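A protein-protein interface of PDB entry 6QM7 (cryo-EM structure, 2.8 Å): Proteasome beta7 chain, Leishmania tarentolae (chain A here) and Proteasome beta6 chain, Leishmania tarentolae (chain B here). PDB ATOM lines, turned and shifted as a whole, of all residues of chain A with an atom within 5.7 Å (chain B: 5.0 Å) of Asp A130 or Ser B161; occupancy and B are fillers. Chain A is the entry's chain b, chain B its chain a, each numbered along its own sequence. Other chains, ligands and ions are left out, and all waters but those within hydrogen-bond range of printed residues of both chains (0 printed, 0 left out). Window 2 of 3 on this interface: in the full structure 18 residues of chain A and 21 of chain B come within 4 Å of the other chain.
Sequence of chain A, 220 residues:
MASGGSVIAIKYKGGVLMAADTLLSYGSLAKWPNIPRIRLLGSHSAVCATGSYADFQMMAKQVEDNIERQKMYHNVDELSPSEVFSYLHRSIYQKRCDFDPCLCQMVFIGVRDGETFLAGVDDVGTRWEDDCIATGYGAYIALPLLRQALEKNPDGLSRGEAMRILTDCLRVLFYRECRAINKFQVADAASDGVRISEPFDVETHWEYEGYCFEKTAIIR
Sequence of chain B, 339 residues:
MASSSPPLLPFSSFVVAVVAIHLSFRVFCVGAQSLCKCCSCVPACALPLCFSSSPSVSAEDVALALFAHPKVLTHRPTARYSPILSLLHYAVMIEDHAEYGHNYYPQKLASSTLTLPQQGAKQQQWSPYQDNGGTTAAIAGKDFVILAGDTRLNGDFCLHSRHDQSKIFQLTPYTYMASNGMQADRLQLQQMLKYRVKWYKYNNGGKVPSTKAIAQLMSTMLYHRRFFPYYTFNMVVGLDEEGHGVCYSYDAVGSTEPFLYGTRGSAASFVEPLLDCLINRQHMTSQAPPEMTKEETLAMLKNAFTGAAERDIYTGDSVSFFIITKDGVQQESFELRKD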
ATOM      1  N   LYS A  11      22.885  12.655  20.411  1.00  0.00           N
ATOM      2  CA  LYS A  11      24.039  12.407  19.520  1.00  0.00           C
ATOM      3  C   LYS A  11      25.316  12.747  20.275  1.00  0.00           C
ATOM      4  O   LYS A  11      25.324  13.722  21.054  1.00  0.00           O
ATOM      5  CB  LYS A  11      23.951  13.228  18.237  1.00  0.00           C
ATOM      6  CG  LYS A  11      22.911  12.716  17.255  1.00  0.00           C
ATOM      7  CD  LYS A  11      22.601  13.708  16.178  1.00  0.00           C
ATOM      8  CE  LYS A  11      22.378  13.102  14.812  1.00  0.00           C
ATOM      9  NZ  LYS A  11      21.438  13.934  14.022  1.00  0.00           N
ATOM     10  N   LEU A 118      18.995  10.626  14.387  1.00  0.00           N
ATOM     11  CA  LEU A 118      18.208  10.653  15.634  1.00  0.00           C
ATOM     12  C   LEU A 118      16.973  11.497  15.370  1.00  0.00           C
ATOM     13  O   LEU A 118      17.111  12.580  14.831  1.00  0.00           O
ATOM     14  CB  LEU A 118      19.068  11.246  16.742  1.00  0.00           C
ATOM     15  CG  LEU A 118      18.285  11.763  17.938  1.00  0.00           C
ATOM     16  CD1 LEU A 118      17.611  10.630  18.693  1.00  0.00           C
ATOM     17  CD2 LEU A 118      19.183  12.537  18.875  1.00  0.00           C
ATOM     18  N   ALA A 119      15.810  11.001  15.727  1.00  0.00           N
ATOM     19  CA  ALA A 119      14.526  11.615  15.370  1.00  0.00           C
ATOM     20  C   ALA A 119      13.451  11.139  16.331  1.00  0.00           C
ATOM     21  O   ALA A 119      13.587  10.035  16.850  1.00  0.00           O
ATOM     22  CB  ALA A 119      14.175  11.235  13.962  1.00  0.00           C
ATOM     23  N   TRP A 128      10.615  15.105  13.944  1.00  0.00           N
ATOM     24  CA  TRP A 128      11.686  16.107  14.113  1.00  0.00           C
ATOM     25  C   TRP A 128      13.003  15.385  14.349  1.00  0.00           C
ATOM     26  O   TRP A 128      13.020  14.450  15.134  1.00  0.00           O
ATOM     27  CB  TRP A 128      11.334  17.092  15.229  1.00  0.00           C
ATOM     28  CG  TRP A 128      11.241  16.488  16.590  1.00  0.00           C
ATOM     29  CD1 TRP A 128      12.213  16.493  17.538  1.00  0.00           C
ATOM     30  CD2 TRP A 128      10.123  15.802  17.172  1.00  0.00           C
ATOM     31  NE1 TRP A 128      11.794  15.824  18.651  1.00  0.00           N
ATOM     32  CE2 TRP A 128      10.520  15.385  18.456  1.00  0.00           C
ATOM     33  CE3 TRP A 128       8.836  15.475  16.733  1.00  0.00           C
ATOM     34  CZ2 TRP A 128       9.683  14.670  19.307  1.00  0.00           C
ATOM     35  CZ3 TRP A 128       8.000  14.769  17.576  1.00  0.00           C
ATOM     36  CH2 TRP A 128       8.419  14.381  18.852  1.00  0.00           C
ATOM     37  N   GLU A 129      14.026  15.768  13.596  1.00  0.00           N
ATOM     38  CA  GLU A 129      15.418  15.336  13.821  1.00  0.00           C
ATOM     39  C   GLU A 129      16.051  16.402  14.698  1.00  0.00           C
ATOM     40  O   GLU A 129      15.653  17.564  14.581  1.00  0.00           O
ATOM     41  CB  GLU A 129      16.176  15.199  12.509  1.00  0.00           C
ATOM     42  CG  GLU A 129      15.451  14.397  11.441  1.00  0.00           C
ATOM     43  CD  GLU A 129      16.250  14.210  10.150  1.00  0.00           C
ATOM     44  OE1 GLU A 129      15.621  13.939   9.089  1.00  0.00           O
ATOM     45  OE2 GLU A 129      17.510  14.322  10.195  1.00  0.00           O
ATOM     46  N   ASP A 130      16.965  16.004  15.571  1.00  0.00           N
ATOM     47  CA  ASP A 130      17.698  16.953  16.439  1.00  0.00           C
ATOM     48  C   ASP A 130      18.902  16.239  17.032  1.00  0.00           C
ATOM     49  O   ASP A 130      18.961  15.015  16.902  1.00  0.00           O
ATOM     50  CB  ASP A 130      16.781  17.526  17.518  1.00  0.00           C
ATOM     51  CG  ASP A 130      17.016  19.004  17.764  1.00  0.00           C
ATOM     52  OD1 ASP A 130      18.199  19.399  17.913  1.00  0.00           O
ATOM     53  OD2 ASP A 130      16.016  19.748  17.771  1.00  0.00           O
ATOM     54  N   ASP A 131      19.816  16.987  17.649  1.00  0.00           N
ATOM     55  CA  ASP A 131      21.017  16.414  18.309  1.00  0.00           C
ATOM     56  C   ASP A 131      20.627  15.787  19.647  1.00  0.00           C
ATOM     57  O   ASP A 131      21.442  15.018  20.180  1.00  0.00           O
ATOM     58  CB  ASP A 131      22.129  17.450  18.467  1.00  0.00           C
ATOM     59  CG  ASP A 131      22.898  17.712  17.187  1.00  0.00           C
ATOM     60  OD1 ASP A 131      22.530  17.123  16.144  1.00  0.00           O
ATOM     61  OD2 ASP A 131      23.863  18.508  17.245  1.00  0.00           O
ATOM     62  N   CYS A 132      19.447  16.111  20.178  1.00  0.00           N
ATOM     63  CA  CYS A 132      18.862  15.408  21.346  1.00  0.00           C
ATOM     64  C   CYS A 132      17.343  15.401  21.253  1.00  0.00           C
ATOM     65  O   CYS A 132      16.757  16.395  20.864  1.00  0.00           O
ATOM     66  CB  CYS A 132      19.276  16.067  22.649  1.00  0.00           C
ATOM     67  SG  CYS A 132      18.608  17.737  22.781  1.00  0.00           S
ATOM     68  N   ILE A 133      16.759  14.276  21.599  1.00  0.00           N
ATOM     69  CA  ILE A 133      15.308  13.999  21.501  1.00  0.00           C
ATOM     70  C   ILE A 133      14.890  13.425  22.836  1.00  0.00           C
ATOM     71  O   ILE A 133      15.656  12.625  23.388  1.00  0.00           O
ATOM     72  CB  ILE A 133      15.030  12.965  20.398  1.00  0.00           C
ATOM     73  CG1 ILE A 133      15.540  13.419  19.033  1.00  0.00           C
ATOM     74  CG2 ILE A 133      13.548  12.614  20.355  1.00  0.00           C
ATOM     75  CD1 ILE A 133      14.724  14.515  18.417  1.00  0.00           C
ATOM     76  N   ARG A 147      20.002  19.650  26.020  1.00  0.00           N
ATOM     77  CA  ARG A 147      20.186  20.846  25.164  1.00  0.00           C
ATOM     78  C   ARG A 147      21.293  21.737  25.729  1.00  0.00           C
ATOM     79  O   ARG A 147      22.108  22.233  24.934  1.00  0.00           O
ATOM     80  CB  ARG A 147      18.886  21.638  25.083  1.00  0.00           C
ATOM     81  CG  ARG A 147      17.815  20.934  24.278  1.00  0.00           C
ATOM     82  CD  ARG A 147      16.933  21.954  23.639  1.00  0.00           C
ATOM     83  NE  ARG A 147      15.888  21.283  22.894  1.00  0.00           N
ATOM     84  CZ  ARG A 147      14.611  21.235  23.240  1.00  0.00           C
ATOM     85  NH1 ARG A 147      14.175  21.832  24.343  1.00  0.00           N
ATOM     86  NH2 ARG A 147      13.763  20.588  22.455  1.00  0.00           N
ATOM     87  N   THR B 151      11.782  28.640  12.184  1.00  0.00           N
ATOM     88  CA  THR B 151      12.294  27.255  12.189  1.00  0.00           C
ATOM     89  C   THR B 151      11.913  26.538  13.477  1.00  0.00           C
ATOM     90  O   THR B 151      12.246  25.362  13.593  1.00  0.00           O
ATOM     91  CB  THR B 151      13.805  27.258  11.951  1.00  0.00           C
ATOM     92  OG1 THR B 151      14.410  28.047  12.981  1.00  0.00           O
ATOM     93  CG2 THR B 151      14.145  27.786  10.571  1.00  0.00           C
ATOM     94  N   ARG B 152      11.219  27.190  14.398  1.00  0.00           N
ATOM     95  CA  ARG B 152      10.879  26.534  15.681  1.00  0.00           C
ATOM     96  C   ARG B 152       9.624  25.699  15.447  1.00  0.00           C
ATOM     97  O   ARG B 152       8.677  26.199  14.827  1.00  0.00           O
ATOM     98  CB  ARG B 152      10.848  27.559  16.816  1.00  0.00           C
ATOM     99  CG  ARG B 152       9.531  27.743  17.544  1.00  0.00           C
ATOM    100  CD  ARG B 152       9.715  27.559  19.039  1.00  0.00           C
ATOM    101  NE  ARG B 152      10.811  28.369  19.555  1.00  0.00           N
ATOM    102  CZ  ARG B 152      10.691  29.448  20.319  1.00  0.00           C
ATOM    103  NH1 ARG B 152       9.505  29.904  20.697  1.00  0.00           N
ATOM    104  NH2 ARG B 152      11.785  30.074  20.716  1.00  0.00           N
ATOM    105  N   LEU B 153       9.694  24.443  15.870  1.00  0.00           N
ATOM    106  CA  LEU B 153       8.603  23.448  15.851  1.00  0.00           C
ATOM    107  C   LEU B 153       8.273  23.178  17.298  1.00  0.00           C
ATOM    108  O   LEU B 153       9.112  22.578  17.958  1.00  0.00           O
ATOM    109  CB  LEU B 153       9.117  22.181  15.170  1.00  0.00           C
ATOM    110  CG  LEU B 153       8.231  20.943  15.272  1.00  0.00           C
ATOM    111  CD1 LEU B 153       6.975  21.082  14.431  1.00  0.00           C
ATOM    112  CD2 LEU B 153       9.012  19.722  14.829  1.00  0.00           C
ATOM    113  N   LEU B 159       9.146  22.591  23.392  1.00  0.00           N
ATOM    114  CA  LEU B 159       9.559  22.775  21.980  1.00  0.00           C
ATOM    115  C   LEU B 159      10.409  21.577  21.541  1.00  0.00           C
ATOM    116  O   LEU B 159      11.256  21.122  22.314  1.00  0.00           O
ATOM    117  CB  LEU B 159      10.224  24.151  21.803  1.00  0.00           C
ATOM    118  CG  LEU B 159      11.732  24.208  21.551  1.00  0.00           C
ATOM    119  CD1 LEU B 159      12.061  25.302  20.561  1.00  0.00           C
ATOM    120  CD2 LEU B 159      12.497  24.445  22.836  1.00  0.00           C
ATOM    121  N   HIS B 160      10.117  21.071  20.345  1.00  0.00           N
ATOM    122  CA  HIS B 160      10.678  19.835  19.750  1.00  0.00           C
ATOM    123  C   HIS B 160      12.032  20.136  19.115  1.00  0.00           C
ATOM    124  O   HIS B 160      12.994  19.386  19.369  1.00  0.00           O
ATOM    125  CB  HIS B 160       9.729  19.270  18.683  1.00  0.00           C
ATOM    126  CG  HIS B 160       8.487  18.646  19.226  1.00  0.00           C
ATOM    127  ND1 HIS B 160       8.453  18.013  20.458  1.00  0.00           N
ATOM    128  CD2 HIS B 160       7.259  18.495  18.679  1.00  0.00           C
ATOM    129  CE1 HIS B 160       7.238  17.541  20.655  1.00  0.00           C
ATOM    130  NE2 HIS B 160       6.488  17.814  19.575  1.00  0.00           N
ATOM    131  N   SER B 161      12.068  21.161  18.273  1.00  0.00           N
ATOM    132  CA  SER B 161      13.252  21.543  17.477  1.00  0.00           C
ATOM    133  C   SER B 161      13.288  23.051  17.305  1.00  0.00           C
ATOM    134  O   SER B 161      12.224  23.664  17.314  1.00  0.00           O
ATOM    135  CB  SER B 161      13.229  20.847  16.147  1.00  0.00           C
ATOM    136  OG  SER B 161      14.427  21.072  15.412  1.00  0.00           O
ATOM    137  N   ARG B 162      14.488  23.604  17.162  1.00  0.00           N
ATOM    138  CA  ARG B 162      14.733  25.000  16.726  1.00  0.00           C
ATOM    139  C   ARG B 162      15.133  25.026  15.248  1.00  0.00           C
ATOM    140  O   ARG B 162      15.285  26.135  14.716  1.00  0.00           O
ATOM    141  CB  ARG B 162      15.879  25.597  17.542  1.00  0.00           C
ATOM    142  CG  ARG B 162      15.753  25.423  19.047  1.00  0.00           C
ATOM    143  CD  ARG B 162      16.646  26.396  19.799  1.00  0.00           C
ATOM    144  NE  ARG B 162      15.842  27.171  20.734  1.00  0.00           N
ATOM    145  CZ  ARG B 162      15.640  26.880  22.011  1.00  0.00           C
ATOM    146  NH1 ARG B 162      14.864  27.667  22.734  1.00  0.00           N
ATOM    147  NH2 ARG B 162      16.194  25.813  22.567  1.00  0.00           N
ATOM    148  N   HIS B 163      15.329  23.859  14.622  1.00  0.00           N
ATOM    149  CA  HIS B 163      15.953  23.712  13.282  1.00  0.00           C
ATOM    150  C   HIS B 163      14.994  23.038  12.302  1.00  0.00           C
ATOM    151  O   HIS B 163      15.491  22.472  11.310  1.00  0.00           O
ATOM    152  CB  HIS B 163      17.289  22.967  13.409  1.00  0.00           C
ATOM    153  CG  HIS B 163      18.275  23.716  14.238  1.00  0.00           C
ATOM    154  ND1 HIS B 163      18.632  23.303  15.513  1.00  0.00           N
ATOM    155  CD2 HIS B 163      18.939  24.874  14.007  1.00  0.00           C
ATOM    156  CE1 HIS B 163      19.497  24.159  16.024  1.00  0.00           C
ATOM    157  NE2 HIS B 163      19.702  25.134  15.117  1.00  0.00           N
ATOM    158  N   ASP B 164      13.683  23.122  12.543  1.00  0.00           N
ATOM    159  CA  ASP B 164      12.647  22.531  11.656  1.00  0.00           C
ATOM    160  C   ASP B 164      12.562  23.375  10.385  1.00  0.00           C
ATOM    161  O   ASP B 164      12.116  24.524  10.482  1.00  0.00           O
ATOM    162  CB  ASP B 164      11.281  22.424  12.340  1.00  0.00           C
ATOM    163  CG  ASP B 164      10.146  21.987  11.416  1.00  0.00           C
ATOM    164  OD1 ASP B 164       9.126  22.735  11.333  1.00  0.00           O
ATOM    165  OD2 ASP B 164      10.281  20.904  10.789  1.00  0.00           O
ATOM    166  N   ASP B 317      13.792  31.494  17.051  1.00  0.00           N
ATOM    167  CA  ASP B 317      14.961  30.600  16.829  1.00  0.00           C
ATOM    168  C   ASP B 317      15.714  31.074  15.590  1.00  0.00           C
ATOM    169  O   ASP B 317      16.742  31.754  15.769  1.00  0.00           O
ATOM    170  CB  ASP B 317      14.560  29.123  16.882  1.00  0.00           C
ATOM    171  CG  ASP B 317      14.009  28.720  18.251  1.00  0.00           C
ATOM    172  OD1 ASP B 317      13.691  29.623  19.060  1.00  0.00           O
ATOM    173  OD2 ASP B 317      13.890  27.514  18.513  1.00  0.00           O
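Printed residues of chain A that touch a printed residue of chain B: Trp A128, Glu A129, Asp A130 and Arg A147. Of the 10 printed residues of chain B, 4 touch a printed residue of chain A. Hydrophobic or aromatic side chains of chain B within 4 Å of the printed part of chain A: Leu B153, Leu B159 and His B160. Among the printed residues, 7 pairs touch across the chains. Among the printed residues, no Asp or Glu carboxylate lies within 4 Å of a Lys or Arg side-chain nitrogen of the other chain.
Leu A118 touches none of the printed residues of chain B. Of the printed residues of chain B, Trp A128 touches Leu B153 (3.5 Å) and His B160 (3.5 Å). Of the printed residues of chain B, Glu A129 touches Ser B161 (3.8 Å). Asp A130 touches just these residues of chain B: His B160 and Ser B161. Of the printed residues of chain A, His B160 touches Trp A128 (3.5 Å), Asp A130 (3.4 Å) and Arg A147 (3.4 Å). Of chain A, only Glu A129 (3.8 Å) and Asp A130 (3.1 Å) come within 4 Å of Ser B161. The nearest printed residue of chain A that does not touch Leu B159 is Trp A128 (6.5 Å).
The side-chain carboxylate (OD2) of Asp A130 sits close to the backbone carbonyl oxygen (O) of His B160 (3.4 Å). O of Leu B159 lies within hydrogen-bond range of NH2 of Arg A147, at 2.6 Å. The guanidinium group (NH2) of Arg A147 lies within hydrogen-bond range of the backbone carbonyl oxygen (O) of His B160. OG of Ser B161 sits at hydrogen-bond distance from OD2 of Asp A130 (3.1 Å).
O of Leu B153 lies within hydrogen-bond range of N of His B160 (3.0 Å). OG of Ser B161 lies within hydrogen-bond range of N of His B163, at 3.0 Å. The backbone NH (N) of Leu B153 sits at hydrogen-bond distance from the backbone carbonyl oxygen (O) of Ser B161 (3.0 Å).
CB of Trp A128 touches CD2 of Leu B153 (3.5 Å). His B160 touches Trp A128. OG of Ser B161 touches O of Glu A129, 3.8 Å away.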
